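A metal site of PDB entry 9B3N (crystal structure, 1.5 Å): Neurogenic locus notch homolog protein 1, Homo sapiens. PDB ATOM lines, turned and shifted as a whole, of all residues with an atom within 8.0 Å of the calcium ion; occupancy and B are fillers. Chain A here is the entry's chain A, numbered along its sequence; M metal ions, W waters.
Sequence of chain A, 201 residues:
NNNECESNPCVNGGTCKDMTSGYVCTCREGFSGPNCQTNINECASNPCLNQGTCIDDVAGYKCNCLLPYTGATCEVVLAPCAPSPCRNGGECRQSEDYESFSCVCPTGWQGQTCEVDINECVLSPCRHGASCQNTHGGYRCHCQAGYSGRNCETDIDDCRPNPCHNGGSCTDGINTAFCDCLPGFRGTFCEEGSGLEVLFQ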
ATOM      1  N   ALA A 145      12.824 -13.778   2.583  1.00  0.00           N
ATOM      2  CA  ALA A 145      13.400 -12.746   3.434  1.00  0.00           C
ATOM      3  C   ALA A 145      13.844 -11.533   2.616  1.00  0.00           C
ATOM      4  O   ALA A 145      14.475 -11.669   1.559  1.00  0.00           O
ATOM      5  CB  ALA A 145      14.590 -13.323   4.219  1.00  0.00           C
ATOM      6  N   GLY A 146      13.443 -10.345   3.065  1.00  0.00           N
ATOM      7  CA  GLY A 146      13.793  -9.121   2.389  1.00  0.00           C
ATOM      8  C   GLY A 146      12.689  -8.507   1.558  1.00  0.00           C
ATOM      9  O   GLY A 146      12.849  -7.363   1.089  1.00  0.00           O
ATOM     10  N   TYR A 147      11.581  -9.220   1.326  1.00  0.00           N
ATOM     11  CA  TYR A 147      10.570  -8.732   0.404  1.00  0.00           C
ATOM     12  C   TYR A 147       9.225  -8.653   1.107  1.00  0.00           C
ATOM     13  O   TYR A 147       8.955  -9.381   2.079  1.00  0.00           O
ATOM     14  CB  TYR A 147      10.430  -9.626  -0.809  1.00  0.00           C
ATOM     15  CG  TYR A 147      11.721  -9.540  -1.556  1.00  0.00           C
ATOM     16  CD1 TYR A 147      11.946  -8.509  -2.498  1.00  0.00           C
ATOM     17  CD2 TYR A 147      12.703 -10.500  -1.359  1.00  0.00           C
ATOM     18  CE1 TYR A 147      13.185  -8.396  -3.156  1.00  0.00           C
ATOM     19  CE2 TYR A 147      13.961 -10.442  -2.034  1.00  0.00           C
ATOM     20  CZ  TYR A 147      14.182  -9.414  -2.959  1.00  0.00           C
ATOM     21  OH  TYR A 147      15.390  -9.390  -3.604  1.00  0.00           O
ATOM     22  N   THR A 154       8.159  -5.779  -3.403  1.00  0.00           N
ATOM     23  CA  THR A 154       8.870  -4.684  -2.740  1.00  0.00           C
ATOM     24  C   THR A 154      10.074  -5.191  -1.987  1.00  0.00           C
ATOM     25  O   THR A 154       9.948  -6.044  -1.112  1.00  0.00           O
ATOM     26  CB  THR A 154       7.910  -3.989  -1.794  1.00  0.00           C
ATOM     27  OG1 THR A 154       6.824  -3.520  -2.610  1.00  0.00           O
ATOM     28  CG2 THR A 154       8.598  -2.854  -1.075  1.00  0.00           C
ATOM     29  N   ASP A 155      11.224  -4.616  -2.292  1.00  0.00           N
ATOM     30  CA  ASP A 155      12.424  -4.830  -1.490  1.00  0.00           C
ATOM     31  C   ASP A 155      12.305  -3.983  -0.230  1.00  0.00           C
ATOM     32  O   ASP A 155      12.324  -2.769  -0.286  1.00  0.00           O
ATOM     33  CB  ASP A 155      13.629  -4.455  -2.339  1.00  0.00           C
ATOM     34  CG  ASP A 155      14.990  -4.737  -1.631  1.00  0.00           C
ATOM     35  OD1 ASP A 155      15.055  -4.452  -0.432  1.00  0.00           O
ATOM     36  OD2 ASP A 155      15.888  -5.257  -2.351  1.00  0.00           O
ATOM     37  N   ILE A 156      12.163  -4.631   0.911  1.00  0.00           N
ATOM     38  CA  ILE A 156      11.894  -3.937   2.171  1.00  0.00           C
ATOM     39  C   ILE A 156      12.940  -2.831   2.409  1.00  0.00           C
ATOM     40  O   ILE A 156      14.122  -3.020   2.136  1.00  0.00           O
ATOM     41  CB  ILE A 156      11.882  -4.971   3.317  1.00  0.00           C
ATOM     42  CG1 ILE A 156      10.678  -5.925   3.147  1.00  0.00           C
ATOM     43  CG2 ILE A 156      11.984  -4.334   4.729  1.00  0.00           C
ATOM     44  CD1 ILE A 156      10.760  -7.045   4.132  1.00  0.00           C
ATOM     45  N   ASP A 157      12.505  -1.669   2.930  1.00  0.00           N
ATOM     46  CA  ASP A 157      13.472  -0.608   3.256  1.00  0.00           C
ATOM     47  C   ASP A 157      14.121  -0.921   4.600  1.00  0.00           C
ATOM     48  O   ASP A 157      13.558  -0.643   5.666  1.00  0.00           O
ATOM     49  CB  ASP A 157      12.781   0.761   3.298  1.00  0.00           C
ATOM     50  CG  ASP A 157      13.738   1.894   3.454  1.00  0.00           C
ATOM     51  OD1 ASP A 157      14.947   1.621   3.630  1.00  0.00           O
ATOM     52  OD2 ASP A 157      13.296   3.057   3.373  1.00  0.00           O
ATOM     53  N   ASP A 158      15.307  -1.517   4.522  1.00  0.00           N
ATOM     54  CA  ASP A 158      16.038  -1.844   5.744  1.00  0.00           C
ATOM     55  C   ASP A 158      16.653  -0.636   6.405  1.00  0.00           C
ATOM     56  O   ASP A 158      17.230  -0.795   7.470  1.00  0.00           O
ATOM     57  CB  ASP A 158      17.107  -2.885   5.448  1.00  0.00           C
ATOM     58  CG  ASP A 158      16.475  -4.236   5.035  1.00  0.00           C
ATOM     59  OD1 ASP A 158      15.851  -4.871   5.899  1.00  0.00           O
ATOM     60  OD2 ASP A 158      16.561  -4.624   3.864  1.00  0.00           O
ATOM     61  N   CYS A 159      16.457   0.561   5.846  1.00  0.00           N
ATOM     62  CA  CYS A 159      17.016   1.755   6.420  1.00  0.00           C
ATOM     63  C   CYS A 159      15.982   2.567   7.182  1.00  0.00           C
ATOM     64  O   CYS A 159      16.308   3.669   7.645  1.00  0.00           O
ATOM     65  CB  CYS A 159      17.626   2.594   5.323  1.00  0.00           C
ATOM     66  SG  CYS A 159      19.159   1.774   4.775  1.00  0.00           S
ATOM     67  N   THR A 171      22.520   2.530   3.741  1.00  0.00           N
ATOM     68  CA  THR A 171      22.235   2.078   2.366  1.00  0.00           C
ATOM     69  C   THR A 171      21.502   0.767   2.429  1.00  0.00           C
ATOM     70  O   THR A 171      21.926  -0.177   3.120  1.00  0.00           O
ATOM     71  CB  THR A 171      23.517   1.897   1.541  1.00  0.00           C
ATOM     72  OG1 THR A 171      24.232   3.126   1.496  1.00  0.00           O
ATOM     73  CG2 THR A 171      23.226   1.436   0.098  1.00  0.00           C
ATOM     74  N   ASP A 172      20.393   0.682   1.710  1.00  0.00           N
ATOM     75  CA  ASP A 172      19.588  -0.522   1.727  1.00  0.00           C
ATOM     76  C   ASP A 172      20.168  -1.563   0.761  1.00  0.00           C
ATOM     77  O   ASP A 172      20.632  -1.252  -0.322  1.00  0.00           O
ATOM     78  CB  ASP A 172      18.164  -0.188   1.303  1.00  0.00           C
ATOM     79  CG  ASP A 172      17.276  -1.397   1.299  1.00  0.00           C
ATOM     80  OD1 ASP A 172      17.083  -2.019   2.373  1.00  0.00           O
ATOM     81  OD2 ASP A 172      16.823  -1.765   0.219  1.00  0.00           O
ATOM     82  N   GLY A 173      19.984  -2.852   1.115  1.00  0.00           N
ATOM     83  CA  GLY A 173      20.264  -3.946   0.228  1.00  0.00           C
ATOM     84  C   GLY A 173      19.200  -5.019   0.298  1.00  0.00           C
ATOM     85  O   GLY A 173      18.203  -4.781   0.982  1.00  0.00           O
ATOM     86  N   ILE A 174      19.446  -6.194  -0.239  1.00  0.00           N
ATOM     87  CA  ILE A 174      18.478  -7.297  -0.152  1.00  0.00           C
ATOM     88  C   ILE A 174      18.645  -7.885   1.256  1.00  0.00           C
ATOM     89  O   ILE A 174      19.682  -8.466   1.585  1.00  0.00           O
ATOM     90  CB  ILE A 174      18.707  -8.351  -1.237  1.00  0.00           C
ATOM     91  CG1 ILE A 174      18.637  -7.689  -2.604  1.00  0.00           C
ATOM     92  CG2 ILE A 174      17.691  -9.482  -1.112  1.00  0.00           C
ATOM     93  CD1 ILE A 174      19.045  -8.592  -3.723  1.00  0.00           C
ATOM     94  N   ASN A 175      17.647  -7.660   2.093  1.00  0.00           N
ATOM     95  CA  ASN A 175      17.621  -8.117   3.480  1.00  0.00           C
ATOM     96  C   ASN A 175      18.875  -7.676   4.227  1.00  0.00           C
ATOM     97  O   ASN A 175      19.459  -8.455   4.971  1.00  0.00           O
ATOM     98  CB  ASN A 175      17.479  -9.627   3.571  1.00  0.00           C
ATOM     99  CG  ASN A 175      16.944 -10.079   4.932  1.00  0.00           C
ATOM    100  OD1 ASN A 175      16.212  -9.340   5.595  1.00  0.00           O
ATOM    101  ND2 ASN A 175      17.357 -11.273   5.362  1.00  0.00           N
ATOM    102  N   THR A 176      19.316  -6.460   3.985  1.00  0.00           N
ATOM    103  CA  THR A 176      20.552  -6.021   4.662  1.00  0.00           C
ATOM    104  C   THR A 176      20.605  -4.526   4.560  1.00  0.00           C
ATOM    105  O   THR A 176      19.905  -3.928   3.734  1.00  0.00           O
ATOM    106  CB  THR A 176      21.802  -6.681   4.035  1.00  0.00           C
ATOM    107  OG1 THR A 176      22.959  -6.450   4.874  1.00  0.00           O
ATOM    108  CG2 THR A 176      22.099  -6.119   2.645  1.00  0.00           C
ATOM    109  N   ALA A 177      21.463  -3.943   5.373  1.00  0.00           N
ATOM    110  CA  ALA A 177      21.692  -2.505   5.373  1.00  0.00           C
ATOM    111  C   ALA A 177      23.177  -2.296   5.604  1.00  0.00           C
ATOM    112  O   ALA A 177      23.816  -3.110   6.265  1.00  0.00           O
ATOM    113  CB  ALA A 177      20.964  -1.801   6.493  1.00  0.00           C
HETATM  114 CA    CA M   1      16.105  -3.998   1.490  1.00  0.00          CA
HETATM  115  O   HOH W   1      15.147  -6.241   1.959  1.00  0.00           O
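Water W1 lies within hydrogen-bond range of the backbone carbonyl oxygen of Gly 146 and the backbone NH of Asn 175.
The nearest printed residue that does not touch the calcium ion is Asn 175 (4.02 Å).
O of Gly 146 lies within hydrogen-bond range of N of Ile 156 (2.8 Å). The side-chain sulfur (SG) of Cys 159 lies within hydrogen-bond range of the backbone NH (N) of Asp 172, at 3.5 Å. The backbone NH (N) of Thr 176 sits close to the side-chain carboxylate (OD2) of Asp 158, 3.3 Å away.
The calcium ion is bound by OD1 of Asp 155 (2.2 Å), O of Gly 173 (2.3 Å), O of Ile 156 (2.3 Å), OD1 of Asp 172 (2.4 Å), water W1 (2.5 Å), OD2 of Asp 158 (2.5 Å) and OD2 of Asp 172 (2.7 Å). The calcium ion has seven donor atoms within binding distance.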
